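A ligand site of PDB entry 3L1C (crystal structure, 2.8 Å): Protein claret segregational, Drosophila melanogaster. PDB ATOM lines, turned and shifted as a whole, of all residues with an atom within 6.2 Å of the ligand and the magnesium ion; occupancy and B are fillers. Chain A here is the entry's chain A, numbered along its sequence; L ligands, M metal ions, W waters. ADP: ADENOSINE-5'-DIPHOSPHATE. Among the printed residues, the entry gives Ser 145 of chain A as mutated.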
ATOM      1  N   ARG A  63      17.863   7.286 -12.353  1.00  0.00           N
ATOM      2  CA  ARG A  63      17.663   7.055 -10.933  1.00  0.00           C
ATOM      3  C   ARG A  63      18.939   6.510 -10.318  1.00  0.00           C
ATOM      4  O   ARG A  63      19.313   5.359 -10.535  1.00  0.00           O
ATOM      5  CB  ARG A  63      16.539   6.060 -10.719  1.00  0.00           C
ATOM      6  CG  ARG A  63      16.169   5.789  -9.257  1.00  0.00           C
ATOM      7  CD  ARG A  63      14.988   4.816  -9.250  1.00  0.00           C
ATOM      8  NE  ARG A  63      14.196   4.945  -8.031  1.00  0.00           N
ATOM      9  CZ  ARG A  63      14.603   4.491  -6.863  1.00  0.00           C
ATOM     10  NH1 ARG A  63      15.787   3.882  -6.790  1.00  0.00           N
ATOM     11  NH2 ARG A  63      13.853   4.658  -5.788  1.00  0.00           N
ATOM     12  N   ILE A  64      19.617   7.369  -9.559  1.00  0.00           N
ATOM     13  CA  ILE A  64      20.857   7.017  -8.872  1.00  0.00           C
ATOM     14  C   ILE A  64      20.461   6.482  -7.507  1.00  0.00           C
ATOM     15  O   ILE A  64      19.782   7.168  -6.767  1.00  0.00           O
ATOM     16  CB  ILE A  64      21.735   8.252  -8.687  1.00  0.00           C
ATOM     17  CG1 ILE A  64      22.060   8.871 -10.039  1.00  0.00           C
ATOM     18  CG2 ILE A  64      23.004   7.908  -7.951  1.00  0.00           C
ATOM     19  CD1 ILE A  64      22.831  10.146  -9.900  1.00  0.00           C
ATOM     20  N   ARG A  65      20.901   5.277  -7.174  1.00  0.00           N
ATOM     21  CA  ARG A  65      20.555   4.708  -5.870  1.00  0.00           C
ATOM     22  C   ARG A  65      21.557   5.151  -4.797  1.00  0.00           C
ATOM     23  O   ARG A  65      22.711   5.470  -5.112  1.00  0.00           O
ATOM     24  CB  ARG A  65      20.505   3.174  -5.941  1.00  0.00           C
ATOM     25  CG  ARG A  65      21.874   2.518  -6.070  1.00  0.00           C
ATOM     26  CD  ARG A  65      21.780   1.026  -6.313  1.00  0.00           C
ATOM     27  NE  ARG A  65      23.082   0.373  -6.369  1.00  0.00           N
ATOM     28  CZ  ARG A  65      23.790  -0.012  -5.305  1.00  0.00           C
ATOM     29  NH1 ARG A  65      23.319   0.176  -4.082  1.00  0.00           N
ATOM     30  NH2 ARG A  65      24.967  -0.609  -5.474  1.00  0.00           N
ATOM     31  N   PRO A  66      21.141   5.169  -3.517  1.00  0.00           N
ATOM     32  CA  PRO A  66      22.019   5.570  -2.426  1.00  0.00           C
ATOM     33  C   PRO A  66      23.044   4.489  -2.104  1.00  0.00           C
ATOM     34  O   PRO A  66      22.866   3.325  -2.450  1.00  0.00           O
ATOM     35  CB  PRO A  66      21.045   5.791  -1.272  1.00  0.00           C
ATOM     36  CG  PRO A  66      19.973   4.815  -1.543  1.00  0.00           C
ATOM     37  CD  PRO A  66      19.762   4.990  -3.025  1.00  0.00           C
ATOM     38  N   LEU A  68      25.016   1.631  -0.369  1.00  0.00           N
ATOM     39  CA  LEU A  68      24.604   0.502   0.450  1.00  0.00           C
ATOM     40  C   LEU A  68      25.167   0.530   1.881  1.00  0.00           C
ATOM     41  O   LEU A  68      26.260   1.037   2.120  1.00  0.00           O
ATOM     42  CB  LEU A  68      25.003  -0.807  -0.252  1.00  0.00           C
ATOM     43  CG  LEU A  68      26.191  -0.828  -1.228  1.00  0.00           C
ATOM     44  CD1 LEU A  68      25.826  -0.088  -2.504  1.00  0.00           C
ATOM     45  CD2 LEU A  68      27.435  -0.225  -0.601  1.00  0.00           C
ATOM     46  N   GLU A  69      24.418  -0.030   2.832  1.00  0.00           N
ATOM     47  CA  GLU A  69      24.863  -0.069   4.220  1.00  0.00           C
ATOM     48  C   GLU A  69      25.885  -1.185   4.428  1.00  0.00           C
ATOM     49  O   GLU A  69      26.371  -1.415   5.533  1.00  0.00           O
ATOM     50  CB  GLU A  69      23.671  -0.271   5.156  1.00  0.00           C
ATOM     51  CG  GLU A  69      22.664   0.879   5.152  1.00  0.00           C
ATOM     52  CD  GLU A  69      21.740   0.866   3.945  1.00  0.00           C
ATOM     53  OE1 GLU A  69      20.882  -0.037   3.844  1.00  0.00           O
ATOM     54  OE2 GLU A  69      21.871   1.771   3.082  1.00  0.00           O
ATOM     55  N   PRO A 113      19.744   9.926  -5.062  1.00  0.00           N
ATOM     56  CA  PRO A 113      19.640   8.839  -4.075  1.00  0.00           C
ATOM     57  C   PRO A 113      18.581   9.061  -3.013  1.00  0.00           C
ATOM     58  O   PRO A 113      18.269   8.158  -2.242  1.00  0.00           O
ATOM     59  CB  PRO A 113      21.041   8.787  -3.482  1.00  0.00           C
ATOM     60  CG  PRO A 113      21.891   9.180  -4.623  1.00  0.00           C
ATOM     61  CD  PRO A 113      21.140  10.394  -5.140  1.00  0.00           C
ATOM     62  N   SER A 115      15.494  10.361  -3.806  1.00  0.00           N
ATOM     63  CA  SER A 115      14.202  10.234  -4.434  1.00  0.00           C
ATOM     64  C   SER A 115      13.573   8.951  -3.937  1.00  0.00           C
ATOM     65  O   SER A 115      14.197   7.894  -3.951  1.00  0.00           O
ATOM     66  CB  SER A 115      14.361  10.229  -5.932  1.00  0.00           C
ATOM     67  OG  SER A 115      14.882  11.483  -6.370  1.00  0.00           O
ATOM     68  N   GLN A 117      10.396   5.981  -3.668  1.00  0.00           N
ATOM     69  CA  GLN A 117       9.623   5.159  -4.582  1.00  0.00           C
ATOM     70  C   GLN A 117       8.391   5.952  -5.032  1.00  0.00           C
ATOM     71  O   GLN A 117       7.986   5.841  -6.186  1.00  0.00           O
ATOM     72  CB  GLN A 117       9.141   3.882  -3.904  1.00  0.00           C
ATOM     73  CG  GLN A 117      10.236   2.982  -3.374  1.00  0.00           C
ATOM     74  CD  GLN A 117      10.998   2.275  -4.452  1.00  0.00           C
ATOM     75  OE1 GLN A 117      11.559   2.906  -5.356  1.00  0.00           O
ATOM     76  NE2 GLN A 117      11.036   0.957  -4.368  1.00  0.00           N
ATOM     77  N   GLY A 143      19.862  -0.756 -16.736  1.00  0.00           N
ATOM     78  CA  GLY A 143      21.004  -0.494 -15.858  1.00  0.00           C
ATOM     79  C   GLY A 143      21.874  -1.717 -15.641  1.00  0.00           C
ATOM     80  O   GLY A 143      21.481  -2.820 -16.007  1.00  0.00           O
ATOM     81  N   GLN A 144      23.057  -1.541 -15.048  1.00  0.00           N
ATOM     82  CA  GLN A 144      23.954  -2.667 -14.801  1.00  0.00           C
ATOM     83  C   GLN A 144      23.503  -3.398 -13.543  1.00  0.00           C
ATOM     84  O   GLN A 144      22.742  -2.853 -12.753  1.00  0.00           O
ATOM     85  CB  GLN A 144      25.402  -2.195 -14.610  1.00  0.00           C
ATOM     86  CG  GLN A 144      25.699  -1.563 -13.247  1.00  0.00           C
ATOM     87  CD  GLN A 144      27.111  -0.994 -13.138  1.00  0.00           C
ATOM     88  OE1 GLN A 144      28.102  -1.729 -13.102  1.00  0.00           O
ATOM     89  NE2 GLN A 144      27.209   0.337 -13.091  1.00  0.00           N
ATOM     90  N   SER A 145      23.977  -4.627 -13.350  1.00  0.00           N
ATOM     91  CA  SER A 145      23.606  -5.387 -12.166  1.00  0.00           C
ATOM     92  C   SER A 145      23.987  -4.580 -10.936  1.00  0.00           C
ATOM     93  O   SER A 145      25.151  -4.240 -10.745  1.00  0.00           O
ATOM     94  CB  SER A 145      24.327  -6.741 -12.120  1.00  0.00           C
ATOM     95  OG  SER A 145      23.826  -7.645 -13.093  1.00  0.00           O
ATOM     96  N   GLY A 146      22.996  -4.266 -10.114  1.00  0.00           N
ATOM     97  CA  GLY A 146      23.235  -3.503  -8.896  1.00  0.00           C
ATOM     98  C   GLY A 146      22.770  -2.054  -8.950  1.00  0.00           C
ATOM     99  O   GLY A 146      22.606  -1.430  -7.903  1.00  0.00           O
ATOM    100  N   SER A 147      22.534  -1.530 -10.156  1.00  0.00           N
ATOM    101  CA  SER A 147      22.106  -0.151 -10.339  1.00  0.00           C
ATOM    102  C   SER A 147      20.803   0.170  -9.613  1.00  0.00           C
ATOM    103  O   SER A 147      20.574   1.305  -9.208  1.00  0.00           O
ATOM    104  CB  SER A 147      21.943   0.171 -11.828  1.00  0.00           C
ATOM    105  OG  SER A 147      20.838  -0.519 -12.409  1.00  0.00           O
ATOM    106  N   GLY A 148      19.929  -0.828  -9.485  1.00  0.00           N
ATOM    107  CA  GLY A 148      18.676  -0.614  -8.796  1.00  0.00           C
ATOM    108  C   GLY A 148      17.428  -1.000  -9.571  1.00  0.00           C
ATOM    109  O   GLY A 148      16.323  -0.588  -9.197  1.00  0.00           O
ATOM    110  N   LYS A 149      17.577  -1.776 -10.636  1.00  0.00           N
ATOM    111  CA  LYS A 149      16.420  -2.163 -11.441  1.00  0.00           C
ATOM    112  C   LYS A 149      15.321  -2.872 -10.665  1.00  0.00           C
ATOM    113  O   LYS A 149      14.150  -2.513 -10.749  1.00  0.00           O
ATOM    114  CB  LYS A 149      16.856  -3.030 -12.621  1.00  0.00           C
ATOM    115  CG  LYS A 149      17.712  -2.300 -13.638  1.00  0.00           C
ATOM    116  CD  LYS A 149      18.155  -3.219 -14.771  1.00  0.00           C
ATOM    117  CE  LYS A 149      18.968  -4.409 -14.267  1.00  0.00           C
ATOM    118  NZ  LYS A 149      20.302  -4.020 -13.773  1.00  0.00           N
ATOM    119  N   THR A 150      15.690  -3.868  -9.874  1.00  0.00           N
ATOM    120  CA  THR A 150      14.674  -4.598  -9.151  1.00  0.00           C
ATOM    121  C   THR A 150      13.999  -3.779  -8.095  1.00  0.00           C
ATOM    122  O   THR A 150      12.771  -3.785  -7.961  1.00  0.00           O
ATOM    123  CB  THR A 150      15.257  -5.850  -8.545  1.00  0.00           C
ATOM    124  OG1 THR A 150      15.783  -6.651  -9.603  1.00  0.00           O
ATOM    125  CG2 THR A 150      14.200  -6.633  -7.799  1.00  0.00           C
ATOM    126  N   TYR A 151      14.801  -3.056  -7.326  1.00  0.00           N
ATOM    127  CA  TYR A 151      14.266  -2.215  -6.267  1.00  0.00           C
ATOM    128  C   TYR A 151      13.317  -1.163  -6.846  1.00  0.00           C
ATOM    129  O   TYR A 151      12.389  -0.727  -6.184  1.00  0.00           O
ATOM    130  CB  TYR A 151      15.413  -1.565  -5.497  1.00  0.00           C
ATOM    131  CG  TYR A 151      14.922  -0.691  -4.377  1.00  0.00           C
ATOM    132  CD1 TYR A 151      14.517   0.610  -4.621  1.00  0.00           C
ATOM    133  CD2 TYR A 151      14.826  -1.177  -3.062  1.00  0.00           C
ATOM    134  CE1 TYR A 151      14.033   1.417  -3.623  1.00  0.00           C
ATOM    135  CE2 TYR A 151      14.323  -0.362  -2.038  1.00  0.00           C
ATOM    136  CZ  TYR A 151      13.931   0.939  -2.344  1.00  0.00           C
ATOM    137  OH  TYR A 151      13.452   1.809  -1.398  1.00  0.00           O
ATOM    138  N   THR A 152      13.551  -0.770  -8.089  1.00  0.00           N
ATOM    139  CA  THR A 152      12.733   0.214  -8.734  1.00  0.00           C
ATOM    140  C   THR A 152      11.379  -0.361  -9.191  1.00  0.00           C
ATOM    141  O   THR A 152      10.319   0.171  -8.810  1.00  0.00           O
ATOM    142  CB  THR A 152      13.501   0.830  -9.927  1.00  0.00           C
ATOM    143  OG1 THR A 152      14.682   1.478  -9.422  1.00  0.00           O
ATOM    144  CG2 THR A 152      12.650   1.866 -10.645  1.00  0.00           C
ATOM    145  N   VAL A 156      10.816  -3.285  -2.513  1.00  0.00           N
ATOM    146  CA  VAL A 156      10.994  -4.095  -1.318  1.00  0.00           C
ATOM    147  C   VAL A 156       9.766  -3.924  -0.424  1.00  0.00           C
ATOM    148  O   VAL A 156       9.073  -2.915  -0.484  1.00  0.00           O
ATOM    149  CB  VAL A 156      12.269  -3.653  -0.574  1.00  0.00           C
ATOM    150  CG1 VAL A 156      11.905  -2.749   0.605  1.00  0.00           C
ATOM    151  CG2 VAL A 156      13.074  -4.866  -0.156  1.00  0.00           C
ATOM    152  N   SER A 260      18.579 -12.275 -12.957  1.00  0.00           N
ATOM    153  CA  SER A 260      20.047 -12.245 -12.994  1.00  0.00           C
ATOM    154  C   SER A 260      20.596 -11.721 -14.334  1.00  0.00           C
ATOM    155  O   SER A 260      21.006 -10.555 -14.415  1.00  0.00           O
ATOM    156  CB  SER A 260      20.621 -13.650 -12.681  1.00  0.00           C
ATOM    157  OG  SER A 260      20.211 -14.619 -13.620  1.00  0.00           O
ATOM    158  N   ASP A 289      11.782  -5.580 -16.299  1.00  0.00           N
ATOM    159  CA  ASP A 289      12.979  -5.487 -15.451  1.00  0.00           C
ATOM    160  C   ASP A 289      14.115  -6.014 -16.308  1.00  0.00           C
ATOM    161  O   ASP A 289      14.523  -7.157 -16.160  1.00  0.00           O
ATOM    162  CB  ASP A 289      12.849  -6.373 -14.205  1.00  0.00           C
ATOM    163  CG  ASP A 289      13.995  -6.189 -13.202  1.00  0.00           C
ATOM    164  OD1 ASP A 289      15.153  -5.906 -13.619  1.00  0.00           O
ATOM    165  OD2 ASP A 289      13.742  -6.346 -11.993  1.00  0.00           O
ATOM    166  N   LEU A 290      14.616  -5.178 -17.214  1.00  0.00           N
ATOM    167  CA  LEU A 290      15.689  -5.574 -18.096  1.00  0.00           C
ATOM    168  C   LEU A 290      16.874  -6.159 -17.360  1.00  0.00           C
ATOM    169  O   LEU A 290      17.142  -5.788 -16.210  1.00  0.00           O
ATOM    170  CB  LEU A 290      16.143  -4.400 -18.931  1.00  0.00           C
ATOM    171  CG  LEU A 290      15.009  -3.759 -19.718  1.00  0.00           C
ATOM    172  CD1 LEU A 290      15.533  -2.521 -20.446  1.00  0.00           C
ATOM    173  CD2 LEU A 290      14.411  -4.759 -20.678  1.00  0.00           C
ATOM    174  N   ASN A 355      18.681   3.042 -14.232  1.00  0.00           N
ATOM    175  CA  ASN A 355      19.267   2.984 -12.902  1.00  0.00           C
ATOM    176  C   ASN A 355      20.778   3.079 -13.009  1.00  0.00           C
ATOM    177  O   ASN A 355      21.357   2.621 -13.991  1.00  0.00           O
ATOM    178  CB  ASN A 355      18.904   1.678 -12.184  1.00  0.00           C
ATOM    179  CG  ASN A 355      17.426   1.542 -11.947  1.00  0.00           C
ATOM    180  OD1 ASN A 355      16.674   1.205 -12.848  1.00  0.00           O
ATOM    181  ND2 ASN A 355      16.990   1.801 -10.726  1.00  0.00           N
HETATM  182  PB  ADP L   1      19.699  -4.536 -10.176  1.00  0.00           P
HETATM  183  O1B ADP L   1      20.486  -5.795 -10.351  1.00  0.00           O
HETATM  184  O2B ADP L   1      20.291  -3.297 -11.065  1.00  0.00           O
HETATM  185  O3B ADP L   1      18.274  -4.771 -10.542  1.00  0.00           O
HETATM  186  PA  ADP L   1      18.919  -4.233  -7.430  1.00  0.00           P
HETATM  187  O1A ADP L   1      18.211  -2.987  -7.145  1.00  0.00           O
HETATM  188  O2A ADP L   1      17.993  -5.329  -7.662  1.00  0.00           O
HETATM  189  O3A ADP L   1      19.823  -4.059  -8.703  1.00  0.00           O
HETATM  190  O5' ADP L   1      19.947  -4.598  -6.271  1.00  0.00           O
HETATM  191  C5' ADP L   1      20.979  -3.676  -5.843  1.00  0.00           C
HETATM  192  C4' ADP L   1      20.898  -3.486  -4.299  1.00  0.00           C
HETATM  193  O4' ADP L   1      20.759  -2.097  -4.045  1.00  0.00           O
HETATM  194  C3' ADP L   1      19.709  -4.140  -3.614  1.00  0.00           C
HETATM  195  O3' ADP L   1      20.047  -4.663  -2.331  1.00  0.00           O
HETATM  196  C2' ADP L   1      18.701  -3.046  -3.410  1.00  0.00           C
HETATM  197  O2' ADP L   1      17.830  -3.269  -2.287  1.00  0.00           O
HETATM  198  C1' ADP L   1      19.574  -1.827  -3.289  1.00  0.00           C
HETATM  199  N9  ADP L   1      18.936  -0.568  -3.802  1.00  0.00           N
HETATM  200  C8  ADP L   1      18.850  -0.216  -5.103  1.00  0.00           C
HETATM  201  N7  ADP L   1      18.256   0.959  -5.218  1.00  0.00           N
HETATM  202  C5  ADP L   1      17.945   1.386  -4.009  1.00  0.00           C
HETATM  203  C6  ADP L   1      17.312   2.515  -3.489  1.00  0.00           C
HETATM  204  N6  ADP L   1      16.875   3.472  -4.313  1.00  0.00           N
HETATM  205  N1  ADP L   1      17.146   2.650  -2.131  1.00  0.00           N
HETATM  206  C2  ADP L   1      17.584   1.702  -1.267  1.00  0.00           C
HETATM  207  N3  ADP L   1      18.187   0.598  -1.769  1.00  0.00           N
HETATM  208  C4  ADP L   1      18.386   0.403  -3.094  1.00  0.00           C
HETATM  209 MG    MG M   1      17.542  -7.500 -10.947  1.00  0.00          MG
HETATM  210  O   HOH W   1      21.606  -7.433  -7.991  1.00  0.00           O
HETATM  211  O   HOH W   2      16.982  -6.650  -4.802  1.00  0.00           O
HETATM  212  O   HOH W   3      17.984  -7.569  -8.518  1.00  0.00           O
HETATM  213  O   HOH W   4      20.882  -7.152 -13.302  1.00  0.00           O
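The magnesium ion is bound by OG1 of Thr 150 (2.4 Å).
Water W3 binds the magnesium ion, 2.5 Å away.
The magnesium ion has two donor atoms within binding distance.
Water W4 lies within hydrogen-bond range of OG of Ser 145 (3.0 Å), NZ of Lys 149 (3.2 Å) and O1B of the ligand (3.3 Å).
The backbone carbonyl oxygen of Gln 144 is in hydrogen-bond range of the side-chain amino group of Lys 149 (2.9 Å).
The guanidinium group (NE) of Arg 65 lies within hydrogen-bond range of the backbone carbonyl oxygen (O) of Gly 146 (2.4 Å).
NH2 of Arg 63 sits at hydrogen-bond distance from OE1 of Gln 117.
The side-chain hydroxyl (OG1) of Thr 152 lies within hydrogen-bond range of the backbone carbonyl oxygen (O) of Gly 148.
The backbone carbonyl oxygen (O) of Tyr 151 is in hydrogen-bond range of the side-chain amide nitrogen (NE2) of Gln 117 (2.8 Å).
The backbone carbonyl oxygen of Gly 148 is in hydrogen-bond range of the side-chain amide nitrogen of Asn 355 (2.9 Å).
The side-chain amino group of Lys 149 is in hydrogen-bond range of the backbone carbonyl oxygen of Gly 143 (2.8 Å).
OG1 of Thr 150 sits close to OD2 of Asp 289 (3.2 Å).
Merely in contact with the magnesium ion: Asp 289 (3.9 Å).
Two residues have an atom within 4 Å of the magnesium ion: Thr 150 and Asp 289.
Residues that only touch the ligand: Pro 66 (3.5 Å) and Ser 145 (3.6 Å).
Hydrophobic or aromatic side chains within 4 Å of the ligand: Pro 66 and Tyr 151.
Within 4 Å of the ligand: Arg 63, Arg 65, Pro 66, Gln 144, Ser 145, Gly 146, Ser 147, Gly 148, Lys 149, Thr 150 and Tyr 151.
The backbone NH (N) of Ser 147 lies within hydrogen-bond range of an oxygen (O2B) of the ligand.
The side-chain amino group of Lys 149 lies within salt-bridge range of an oxygen (O2B) of the ligand.
O3B of the ligand sits close to N of Lys 149 (3.1 Å).
NH1 of Arg 65 is in hydrogen-bond range of O4' of the ligand (3.4 Å).
NH1 of Arg 63 lies close to N6 of the ligand, 2.7 Å away.
N of Gly 148 lies within hydrogen-bond range of O2B of the ligand.
OG1 of Thr 150 lies close to O2A of the ligand, 3.2 Å away.
An oxygen (O2B) of the ligand sits at hydrogen-bond distance from the side-chain hydroxyl of Ser 147, 3.1 Å away.
O1B of the ligand lies within hydrogen-bond range of N of Gly 146 (2.9 Å).
The backbone carbonyl oxygen (O) of Gln 144 lies close to an oxygen (O2B) of the ligand, at 3.0 Å.
An oxygen (O3B) of the ligand lies within hydrogen-bond range of the backbone NH (N) of Thr 150, at 2.8 Å.
The backbone NH (N) of Tyr 151 lies within hydrogen-bond range of an oxygen (O1A) of the ligand.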
